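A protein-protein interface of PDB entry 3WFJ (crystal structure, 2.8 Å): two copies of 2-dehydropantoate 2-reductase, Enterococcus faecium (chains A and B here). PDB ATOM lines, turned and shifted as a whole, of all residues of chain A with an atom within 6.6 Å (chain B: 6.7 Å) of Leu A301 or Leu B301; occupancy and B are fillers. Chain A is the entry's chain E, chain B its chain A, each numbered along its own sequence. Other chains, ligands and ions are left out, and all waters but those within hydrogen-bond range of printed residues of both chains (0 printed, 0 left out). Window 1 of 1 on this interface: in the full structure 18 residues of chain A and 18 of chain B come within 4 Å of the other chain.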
ATOM      1  N   LEU A 197     -18.629  21.500  17.331  1.00  0.00           N
ATOM      2  CA  LEU A 197     -19.702  21.513  18.261  1.00  0.00           C
ATOM      3  C   LEU A 197     -20.176  20.077  18.560  1.00  0.00           C
ATOM      4  O   LEU A 197     -20.298  19.677  19.732  1.00  0.00           O
ATOM      5  CB  LEU A 197     -20.830  22.451  17.815  1.00  0.00           C
ATOM      6  CG  LEU A 197     -20.406  23.885  17.586  1.00  0.00           C
ATOM      7  CD1 LEU A 197     -21.527  24.806  17.214  1.00  0.00           C
ATOM      8  CD2 LEU A 197     -19.703  24.497  18.799  1.00  0.00           C
ATOM      9  N   ILE A 200     -17.453  18.034  20.528  1.00  0.00           N
ATOM     10  CA  ILE A 200     -17.133  18.456  21.851  1.00  0.00           C
ATOM     11  C   ILE A 200     -18.312  18.126  22.732  1.00  0.00           C
ATOM     12  O   ILE A 200     -18.122  17.712  23.874  1.00  0.00           O
ATOM     13  CB  ILE A 200     -16.797  19.982  21.879  1.00  0.00           C
ATOM     14  CG1 ILE A 200     -15.416  20.228  21.320  1.00  0.00           C
ATOM     15  CG2 ILE A 200     -16.882  20.539  23.266  1.00  0.00           C
ATOM     16  CD1 ILE A 200     -14.285  19.749  22.202  1.00  0.00           C
ATOM     17  N   LEU A 201     -19.511  18.439  22.261  1.00  0.00           N
ATOM     18  CA  LEU A 201     -20.769  18.225  23.061  1.00  0.00           C
ATOM     19  C   LEU A 201     -21.276  16.749  23.109  1.00  0.00           C
ATOM     20  O   LEU A 201     -22.186  16.420  23.862  1.00  0.00           O
ATOM     21  CB  LEU A 201     -21.905  19.144  22.528  1.00  0.00           C
ATOM     22  CG  LEU A 201     -21.569  20.612  22.730  1.00  0.00           C
ATOM     23  CD1 LEU A 201     -22.574  21.504  22.008  1.00  0.00           C
ATOM     24  CD2 LEU A 201     -21.519  20.999  24.213  1.00  0.00           C
ATOM     25  N   THR A 213     -28.612  27.253  22.760  1.00  0.00           N
ATOM     26  CA  THR A 213     -27.506  28.211  22.397  1.00  0.00           C
ATOM     27  C   THR A 213     -26.816  27.902  21.041  1.00  0.00           C
ATOM     28  O   THR A 213     -25.955  28.684  20.621  1.00  0.00           O
ATOM     29  CB  THR A 213     -26.466  28.249  23.477  1.00  0.00           C
ATOM     30  OG1 THR A 213     -26.064  26.889  23.764  1.00  0.00           O
ATOM     31  CG2 THR A 213     -27.038  28.853  24.725  1.00  0.00           C
ATOM     32  N   MET A 217     -24.045  30.332  19.004  1.00  0.00           N
ATOM     33  CA  MET A 217     -22.710  29.787  18.748  1.00  0.00           C
ATOM     34  C   MET A 217     -22.454  29.727  17.259  1.00  0.00           C
ATOM     35  O   MET A 217     -21.455  30.302  16.771  1.00  0.00           O
ATOM     36  CB  MET A 217     -22.601  28.378  19.369  1.00  0.00           C
ATOM     37  CG  MET A 217     -22.740  28.458  20.888  1.00  0.00           C
ATOM     38  SD  MET A 217     -22.263  26.980  21.743  1.00  0.00           S
ATOM     39  CE  MET A 217     -23.457  25.824  21.101  1.00  0.00           C
ATOM     40  N   ASP A 296     -10.573  30.265  17.853  1.00  0.00           N
ATOM     41  CA  ASP A 296      -9.454  29.945  18.665  1.00  0.00           C
ATOM     42  C   ASP A 296      -9.830  28.873  19.746  1.00  0.00           C
ATOM     43  O   ASP A 296      -9.113  27.871  19.984  1.00  0.00           O
ATOM     44  CB  ASP A 296      -8.905  31.194  19.385  1.00  0.00           C
ATOM     45  CG  ASP A 296      -8.337  32.271  18.427  1.00  0.00           C
ATOM     46  OD1 ASP A 296      -7.966  31.978  17.239  1.00  0.00           O
ATOM     47  OD2 ASP A 296      -8.295  33.466  18.910  1.00  0.00           O
ATOM     48  N   PHE A 297     -10.941  29.115  20.436  1.00  0.00           N
ATOM     49  CA  PHE A 297     -11.299  28.382  21.635  1.00  0.00           C
ATOM     50  C   PHE A 297     -11.795  27.027  21.161  1.00  0.00           C
ATOM     51  O   PHE A 297     -11.520  25.973  21.712  1.00  0.00           O
ATOM     52  CB  PHE A 297     -12.373  29.237  22.343  1.00  0.00           C
ATOM     53  CG  PHE A 297     -12.743  28.786  23.706  1.00  0.00           C
ATOM     54  CD1 PHE A 297     -13.896  29.320  24.290  1.00  0.00           C
ATOM     55  CD2 PHE A 297     -12.015  27.825  24.392  1.00  0.00           C
ATOM     56  CE1 PHE A 297     -14.324  28.925  25.557  1.00  0.00           C
ATOM     57  CE2 PHE A 297     -12.407  27.446  25.638  1.00  0.00           C
ATOM     58  CZ  PHE A 297     -13.570  27.988  26.222  1.00  0.00           C
ATOM     59  N   LEU A 298     -12.539  27.057  20.064  1.00  0.00           N
ATOM     60  CA  LEU A 298     -13.095  25.814  19.566  1.00  0.00           C
ATOM     61  C   LEU A 298     -11.958  24.955  19.141  1.00  0.00           C
ATOM     62  O   LEU A 298     -11.892  23.780  19.492  1.00  0.00           O
ATOM     63  CB  LEU A 298     -14.043  26.065  18.379  1.00  0.00           C
ATOM     64  CG  LEU A 298     -14.788  24.852  17.890  1.00  0.00           C
ATOM     65  CD1 LEU A 298     -15.347  24.006  19.052  1.00  0.00           C
ATOM     66  CD2 LEU A 298     -15.917  25.254  16.966  1.00  0.00           C
ATOM     67  N   THR A 299     -11.032  25.531  18.390  1.00  0.00           N
ATOM     68  CA  THR A 299      -9.797  24.790  18.079  1.00  0.00           C
ATOM     69  C   THR A 299      -9.099  24.203  19.333  1.00  0.00           C
ATOM     70  O   THR A 299      -8.856  23.021  19.400  1.00  0.00           O
ATOM     71  CB  THR A 299      -8.802  25.685  17.298  1.00  0.00           C
ATOM     72  OG1 THR A 299      -9.348  26.007  16.009  1.00  0.00           O
ATOM     73  CG2 THR A 299      -7.509  24.937  17.096  1.00  0.00           C
ATOM     74  N   GLU A 300      -8.837  25.083  20.307  1.00  0.00           N
ATOM     75  CA  GLU A 300      -8.190  24.726  21.636  1.00  0.00           C
ATOM     76  C   GLU A 300      -8.946  23.672  22.372  1.00  0.00           C
ATOM     77  O   GLU A 300      -8.394  22.637  22.717  1.00  0.00           O
ATOM     78  CB  GLU A 300      -7.988  25.954  22.522  1.00  0.00           C
ATOM     79  CG  GLU A 300      -6.953  26.980  22.008  1.00  0.00           C
ATOM     80  CD  GLU A 300      -7.270  28.437  22.352  1.00  0.00           C
ATOM     81  OE1 GLU A 300      -8.298  28.717  22.874  1.00  0.00           O
ATOM     82  OE2 GLU A 300      -6.569  29.371  21.958  1.00  0.00           O
ATOM     83  N   LEU A 301     -10.258  23.783  22.342  1.00  0.00           N
ATOM     84  CA  LEU A 301     -11.088  22.723  22.902  1.00  0.00           C
ATOM     85  C   LEU A 301     -10.932  21.365  22.203  1.00  0.00           C
ATOM     86  O   LEU A 301     -10.835  20.337  22.894  1.00  0.00           O
ATOM     87  CB  LEU A 301     -12.576  23.134  22.921  1.00  0.00           C
ATOM     88  CG  LEU A 301     -12.955  24.207  23.971  1.00  0.00           C
ATOM     89  CD1 LEU A 301     -14.367  24.698  23.740  1.00  0.00           C
ATOM     90  CD2 LEU A 301     -12.902  23.690  25.400  1.00  0.00           C
ATOM     91  N   VAL A 302     -10.925  21.331  20.864  1.00  0.00           N
ATOM     92  CA  VAL A 302     -10.849  20.055  20.131  1.00  0.00           C
ATOM     93  C   VAL A 302      -9.491  19.412  20.344  1.00  0.00           C
ATOM     94  O   VAL A 302      -9.401  18.224  20.503  1.00  0.00           O
ATOM     95  CB  VAL A 302     -11.162  20.267  18.640  1.00  0.00           C
ATOM     96  CG1 VAL A 302     -10.692  19.108  17.746  1.00  0.00           C
ATOM     97  CG2 VAL A 302     -12.662  20.528  18.504  1.00  0.00           C
ATOM     98  N   HIS A 303      -8.426  20.202  20.339  1.00  0.00           N
ATOM     99  CA  HIS A 303      -7.087  19.681  20.619  1.00  0.00           C
ATOM    100  C   HIS A 303      -7.044  19.195  22.004  1.00  0.00           C
ATOM    101  O   HIS A 303      -6.615  18.078  22.230  1.00  0.00           O
ATOM    102  CB  HIS A 303      -5.978  20.702  20.371  1.00  0.00           C
ATOM    103  CG  HIS A 303      -5.687  20.927  18.901  1.00  0.00           C
ATOM    104  ND1 HIS A 303      -5.249  22.137  18.406  1.00  0.00           N
ATOM    105  CD2 HIS A 303      -5.878  20.148  17.807  1.00  0.00           C
ATOM    106  CE1 HIS A 303      -5.203  22.122  17.091  1.00  0.00           C
ATOM    107  NE2 HIS A 303      -5.585  20.924  16.701  1.00  0.00           N
ATOM    108  N   ALA A 304      -7.598  19.944  22.953  1.00  0.00           N
ATOM    109  CA  ALA A 304      -7.600  19.452  24.340  1.00  0.00           C
ATOM    110  C   ALA A 304      -8.315  18.107  24.416  1.00  0.00           C
ATOM    111  O   ALA A 304      -7.835  17.194  25.097  1.00  0.00           O
ATOM    112  CB  ALA A 304      -8.276  20.384  25.280  1.00  0.00           C
ATOM    113  N   LYS A 305      -9.359  17.947  23.598  1.00  0.00           N
ATOM    114  CA  LYS A 305     -10.175  16.725  23.593  1.00  0.00           C
ATOM    115  C   LYS A 305      -9.423  15.541  23.004  1.00  0.00           C
ATOM    116  O   LYS A 305      -9.325  14.482  23.647  1.00  0.00           O
ATOM    117  CB  LYS A 305     -11.420  17.005  22.792  1.00  0.00           C
ATOM    118  CG  LYS A 305     -12.427  15.897  22.805  1.00  0.00           C
ATOM    119  CD  LYS A 305     -12.950  15.593  24.183  1.00  0.00           C
ATOM    120  CE  LYS A 305     -13.985  14.491  24.123  1.00  0.00           C
ATOM    121  NZ  LYS A 305     -14.445  14.100  25.497  1.00  0.00           N
ATOM    122  N   GLU A 306      -8.815  15.756  21.812  1.00  0.00           N
ATOM    123  CA  GLU A 306      -7.787  14.871  21.277  1.00  0.00           C
ATOM    124  C   GLU A 306      -6.832  14.395  22.372  1.00  0.00           C
ATOM    125  O   GLU A 306      -6.618  13.189  22.509  1.00  0.00           O
ATOM    126  CB  GLU A 306      -6.963  15.523  20.112  1.00  0.00           C
ATOM    127  CG  GLU A 306      -7.709  15.689  18.784  1.00  0.00           C
ATOM    128  CD  GLU A 306      -7.046  16.633  17.815  1.00  0.00           C
ATOM    129  OE1 GLU A 306      -6.183  17.401  18.286  1.00  0.00           O
ATOM    130  OE2 GLU A 306      -7.437  16.679  16.601  1.00  0.00           O
ATOM    131  N   LEU B 197     -14.695  23.571  31.824  1.00  0.00           N
ATOM    132  CA  LEU B 197     -13.756  22.787  31.026  1.00  0.00           C
ATOM    133  C   LEU B 197     -13.861  21.292  31.354  1.00  0.00           C
ATOM    134  O   LEU B 197     -14.021  20.456  30.451  1.00  0.00           O
ATOM    135  CB  LEU B 197     -12.315  23.310  31.199  1.00  0.00           C
ATOM    136  CG  LEU B 197     -12.124  24.837  30.885  1.00  0.00           C
ATOM    137  CD1 LEU B 197     -10.693  25.299  31.002  1.00  0.00           C
ATOM    138  CD2 LEU B 197     -12.599  25.129  29.471  1.00  0.00           C
ATOM    139  N   ILE B 200     -17.323  19.947  30.095  1.00  0.00           N
ATOM    140  CA  ILE B 200     -17.509  19.912  28.630  1.00  0.00           C
ATOM    141  C   ILE B 200     -16.614  18.862  27.973  1.00  0.00           C
ATOM    142  O   ILE B 200     -17.088  18.075  27.182  1.00  0.00           O
ATOM    143  CB  ILE B 200     -17.214  21.266  28.018  1.00  0.00           C
ATOM    144  CG1 ILE B 200     -18.364  22.198  28.327  1.00  0.00           C
ATOM    145  CG2 ILE B 200     -17.041  21.144  26.556  1.00  0.00           C
ATOM    146  CD1 ILE B 200     -19.652  21.885  27.595  1.00  0.00           C
ATOM    147  N   LEU B 201     -15.358  18.806  28.408  1.00  0.00           N
ATOM    148  CA  LEU B 201     -14.392  17.817  27.959  1.00  0.00           C
ATOM    149  C   LEU B 201     -14.545  16.386  28.531  1.00  0.00           C
ATOM    150  O   LEU B 201     -13.902  15.432  28.046  1.00  0.00           O
ATOM    151  CB  LEU B 201     -12.984  18.354  28.236  1.00  0.00           C
ATOM    152  CG  LEU B 201     -12.706  19.648  27.457  1.00  0.00           C
ATOM    153  CD1 LEU B 201     -11.375  20.229  27.859  1.00  0.00           C
ATOM    154  CD2 LEU B 201     -12.710  19.432  25.916  1.00  0.00           C
ATOM    155  N   THR B 213      -3.679  22.440  25.575  1.00  0.00           N
ATOM    156  CA  THR B 213      -4.292  23.783  25.455  1.00  0.00           C
ATOM    157  C   THR B 213      -4.938  24.294  26.733  1.00  0.00           C
ATOM    158  O   THR B 213      -5.370  25.467  26.789  1.00  0.00           O
ATOM    159  CB  THR B 213      -5.319  23.806  24.332  1.00  0.00           C
ATOM    160  OG1 THR B 213      -6.229  22.737  24.556  1.00  0.00           O
ATOM    161  CG2 THR B 213      -4.643  23.613  23.016  1.00  0.00           C
ATOM    162  N   MET B 217      -6.383  28.181  27.525  1.00  0.00           N
ATOM    163  CA  MET B 217      -7.775  28.358  27.828  1.00  0.00           C
ATOM    164  C   MET B 217      -7.954  28.965  29.184  1.00  0.00           C
ATOM    165  O   MET B 217      -8.551  30.042  29.345  1.00  0.00           O
ATOM    166  CB  MET B 217      -8.445  27.053  27.739  1.00  0.00           C
ATOM    167  CG  MET B 217      -8.388  26.474  26.300  1.00  0.00           C
ATOM    168  SD  MET B 217      -9.486  25.109  26.022  1.00  0.00           S
ATOM    169  CE  MET B 217      -8.833  23.879  27.154  1.00  0.00           C
ATOM    170  N   ASP B 296     -18.579  33.895  27.290  1.00  0.00           N
ATOM    171  CA  ASP B 296     -19.803  33.736  26.490  1.00  0.00           C
ATOM    172  C   ASP B 296     -19.964  32.294  25.909  1.00  0.00           C
ATOM    173  O   ASP B 296     -21.021  31.593  26.083  1.00  0.00           O
ATOM    174  CB  ASP B 296     -19.839  34.703  25.308  1.00  0.00           C
ATOM    175  CG  ASP B 296     -19.864  36.198  25.728  1.00  0.00           C
ATOM    176  OD1 ASP B 296     -20.218  36.569  26.910  1.00  0.00           O
ATOM    177  OD2 ASP B 296     -19.420  37.014  24.862  1.00  0.00           O
ATOM    178  N   PHE B 297     -18.879  31.831  25.273  1.00  0.00           N
ATOM    179  CA  PHE B 297     -18.893  30.598  24.548  1.00  0.00           C
ATOM    180  C   PHE B 297     -18.933  29.426  25.566  1.00  0.00           C
ATOM    181  O   PHE B 297     -19.687  28.404  25.421  1.00  0.00           O
ATOM    182  CB  PHE B 297     -17.642  30.613  23.672  1.00  0.00           C
ATOM    183  CG  PHE B 297     -17.593  29.617  22.576  1.00  0.00           C
ATOM    184  CD1 PHE B 297     -16.373  29.395  21.957  1.00  0.00           C
ATOM    185  CD2 PHE B 297     -18.700  28.841  22.211  1.00  0.00           C
ATOM    186  CE1 PHE B 297     -16.226  28.359  20.986  1.00  0.00           C
ATOM    187  CE2 PHE B 297     -18.577  27.880  21.256  1.00  0.00           C
ATOM    188  CZ  PHE B 297     -17.338  27.634  20.623  1.00  0.00           C
ATOM    189  N   LEU B 298     -18.171  29.567  26.643  1.00  0.00           N
ATOM    190  CA  LEU B 298     -18.125  28.457  27.640  1.00  0.00           C
ATOM    191  C   LEU B 298     -19.486  28.336  28.274  1.00  0.00           C
ATOM    192  O   LEU B 298     -20.052  27.236  28.332  1.00  0.00           O
ATOM    193  CB  LEU B 298     -17.101  28.729  28.703  1.00  0.00           C
ATOM    194  CG  LEU B 298     -16.855  27.597  29.669  1.00  0.00           C
ATOM    195  CD1 LEU B 298     -16.774  26.248  28.981  1.00  0.00           C
ATOM    196  CD2 LEU B 298     -15.584  27.837  30.487  1.00  0.00           C
ATOM    197  N   THR B 299     -20.093  29.486  28.633  1.00  0.00           N
ATOM    198  CA  THR B 299     -21.488  29.493  29.069  1.00  0.00           C
ATOM    199  C   THR B 299     -22.488  28.829  28.100  1.00  0.00           C
ATOM    200  O   THR B 299     -23.109  27.813  28.418  1.00  0.00           O
ATOM    201  CB  THR B 299     -21.961  30.902  29.331  1.00  0.00           C
ATOM    202  OG1 THR B 299     -21.254  31.423  30.437  1.00  0.00           O
ATOM    203  CG2 THR B 299     -23.424  30.831  29.677  1.00  0.00           C
ATOM    204  N   GLU B 300     -22.474  29.311  26.834  1.00  0.00           N
ATOM    205  CA  GLU B 300     -23.270  28.688  25.717  1.00  0.00           C
ATOM    206  C   GLU B 300     -22.989  27.187  25.569  1.00  0.00           C
ATOM    207  O   GLU B 300     -23.920  26.398  25.460  1.00  0.00           O
ATOM    208  CB  GLU B 300     -23.054  29.431  24.445  1.00  0.00           C
ATOM    209  CG  GLU B 300     -23.566  30.887  24.450  1.00  0.00           C
ATOM    210  CD  GLU B 300     -22.699  31.874  23.647  1.00  0.00           C
ATOM    211  OE1 GLU B 300     -21.675  31.502  23.052  1.00  0.00           O
ATOM    212  OE2 GLU B 300     -23.001  33.092  23.629  1.00  0.00           O
ATOM    213  N   LEU B 301     -21.738  26.770  25.719  1.00  0.00           N
ATOM    214  CA  LEU B 301     -21.407  25.339  25.569  1.00  0.00           C
ATOM    215  C   LEU B 301     -22.024  24.495  26.680  1.00  0.00           C
ATOM    216  O   LEU B 301     -22.625  23.459  26.411  1.00  0.00           O
ATOM    217  CB  LEU B 301     -19.890  25.115  25.482  1.00  0.00           C
ATOM    218  CG  LEU B 301     -19.219  25.500  24.151  1.00  0.00           C
ATOM    219  CD1 LEU B 301     -17.737  25.454  24.284  1.00  0.00           C
ATOM    220  CD2 LEU B 301     -19.578  24.547  23.035  1.00  0.00           C
ATOM    221  N   VAL B 302     -21.947  24.985  27.910  1.00  0.00           N
ATOM    222  CA  VAL B 302     -22.523  24.263  29.066  1.00  0.00           C
ATOM    223  C   VAL B 302     -24.067  24.191  29.013  1.00  0.00           C
ATOM    224  O   VAL B 302     -24.632  23.166  29.271  1.00  0.00           O
ATOM    225  CB  VAL B 302     -22.062  24.906  30.394  1.00  0.00           C
ATOM    226  CG1 VAL B 302     -22.913  24.446  31.589  1.00  0.00           C
ATOM    227  CG2 VAL B 302     -20.584  24.603  30.549  1.00  0.00           C
ATOM    228  N   HIS B 303     -24.706  25.271  28.650  1.00  0.00           N
ATOM    229  CA  HIS B 303     -26.107  25.227  28.429  1.00  0.00           C
ATOM    230  C   HIS B 303     -26.472  24.288  27.297  1.00  0.00           C
ATOM    231  O   HIS B 303     -27.355  23.465  27.467  1.00  0.00           O
ATOM    232  CB  HIS B 303     -26.667  26.610  28.146  1.00  0.00           C
ATOM    233  CG  HIS B 303     -26.712  27.467  29.370  1.00  0.00           C
ATOM    234  ND1 HIS B 303     -26.604  28.835  29.310  1.00  0.00           N
ATOM    235  CD2 HIS B 303     -26.835  27.162  30.682  1.00  0.00           C
ATOM    236  CE1 HIS B 303     -26.706  29.343  30.520  1.00  0.00           C
ATOM    237  NE2 HIS B 303     -26.823  28.346  31.375  1.00  0.00           N
ATOM    238  N   ALA B 304     -25.777  24.365  26.170  1.00  0.00           N
ATOM    239  CA  ALA B 304     -26.089  23.431  25.118  1.00  0.00           C
ATOM    240  C   ALA B 304     -26.001  22.009  25.664  1.00  0.00           C
ATOM    241  O   ALA B 304     -26.796  21.169  25.293  1.00  0.00           O
ATOM    242  CB  ALA B 304     -25.133  23.570  23.962  1.00  0.00           C
ATOM    243  N   LYS B 305     -25.042  21.771  26.562  1.00  0.00           N
ATOM    244  CA  LYS B 305     -24.772  20.441  27.071  1.00  0.00           C
ATOM    245  C   LYS B 305     -25.900  19.974  27.947  1.00  0.00           C
ATOM    246  O   LYS B 305     -26.401  18.869  27.796  1.00  0.00           O
ATOM    247  CB  LYS B 305     -23.457  20.462  27.831  1.00  0.00           C
ATOM    248  CG  LYS B 305     -22.965  19.155  28.347  1.00  0.00           C
ATOM    249  CD  LYS B 305     -22.690  18.180  27.223  1.00  0.00           C
ATOM    250  CE  LYS B 305     -22.168  16.875  27.796  1.00  0.00           C
ATOM    251  NZ  LYS B 305     -21.995  15.841  26.757  1.00  0.00           N
ATOM    252  N   GLU B 306     -26.281  20.830  28.885  1.00  0.00           N
ATOM    253  CA  GLU B 306     -27.537  20.698  29.663  1.00  0.00           C
ATOM    254  C   GLU B 306     -28.701  20.290  28.781  1.00  0.00           C
ATOM    255  O   GLU B 306     -29.331  19.284  29.049  1.00  0.00           O
ATOM    256  CB  GLU B 306     -27.913  22.011  30.415  1.00  0.00           C
ATOM    257  CG  GLU B 306     -27.056  22.352  31.622  1.00  0.00           C
ATOM    258  CD  GLU B 306     -27.259  23.765  32.100  1.00  0.00           C
ATOM    259  OE1 GLU B 306     -27.766  24.565  31.301  1.00  0.00           O
ATOM    260  OE2 GLU B 306     -26.779  24.120  33.241  1.00  0.00           O
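The side-chain amino group (NZ) of Lys A305 is in hydrogen-bond range of the backbone carbonyl oxygen (O) of Leu B201 (2.9 Å). The backbone carbonyl oxygen (O) of Glu A300 lies within hydrogen-bond range of the side-chain hydroxyl (OG1) of Thr B213 (2.8 Å). The side-chain hydroxyl (OG1) of Thr B213 sits close to the backbone NH (N) of Ala A304. The backbone carbonyl oxygen (O) of Glu B300 is in hydrogen-bond range of the side-chain hydroxyl (OG1) of Thr A213 (2.8 Å). N of Ala B304 sits close to OG1 of Thr A213 (3.5 Å). NZ of Lys B305 lies within hydrogen-bond range of O of Leu A201 (3.0 Å). O of Ile A200 lies close to O of Ile B200 (3.5 Å).
Among the printed residues, pairs that only touch across the chains: Leu A201 with Ile B200 (3.96 Å), Leu A201 with Leu B301 (3.5 Å), Leu A201 with Ala B304 (3.8 Å), Met A217 with Phe B297 (3.8 Å), Met A217 with Glu B300 (3.7 Å), Met A217 with Leu B301 (3.8 Å), Phe A297 with Met B217 (3.8 Å), Phe A297 with Phe B297 (3.4 Å), Glu A300 with Met B217 (3.8 Å), Leu A301 with Leu B201 (3.7 Å), Leu A301 with Met B217 (3.8 Å) and Leu A301 with Leu B301 (3.5 Å).
Of the printed residues of chain B, Thr A213 touches Glu B300 and Ala B304. Of the printed residues of chain B, Met A217 touches Phe B297 (3.8 Å), Glu B300 (3.7 Å) and Leu B301 (3.8 Å). Printed residues of chain B within 4 Å of Glu A300: Thr B213 and Met B217. Of the printed residues of chain A, Phe B297 touches Met A217 (3.8 Å) and Phe A297 (3.4 Å). Printed residues of chain A within 4 Å of Glu B300: Thr A213 (2.8 Å) and Met A217 (3.7 Å). Of chain A, only Leu A201 (3.5 Å), Met A217 (3.8 Å) and Leu A301 (3.5 Å) come within 4 Å of Leu B301. The nearest residue of chain B that does not touch Leu A301 is Leu B197 (4.3 Å).
Of the 16 printed residues of chain B, 9 touch a printed residue of chain A. Printed residues of chain B that touch a printed residue of chain A: Ile B200, Leu B201, Thr B213, Met B217, Phe B297, Glu B300, Leu B301, Ala B304 and Lys B305. Of the 16 printed residues of chain A, 9 touch a printed residue of chain B. Printed residues of chain A that touch a printed residue of chain B: Ile A200, Leu A201, Thr A213, Met A217, Phe A297, Glu A300, Leu A301, Ala A304 and Lys A305. Hydrophobic or aromatic side chains of chain A within 4 Å of the printed part of chain B: Ile A200, Leu A201, Met A217, Phe A297, Leu A301 and Ala A304.
Ile A200 touches its own counterpart, Ile B200. Leu A201 touches Lys B305, and with the chains exchanged Lys A305 touches Leu B201. Met A217 touches Glu B300, and with the chains exchanged Glu A300 touches Met B217. Phe A297 touches its own counterpart, Phe B297.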
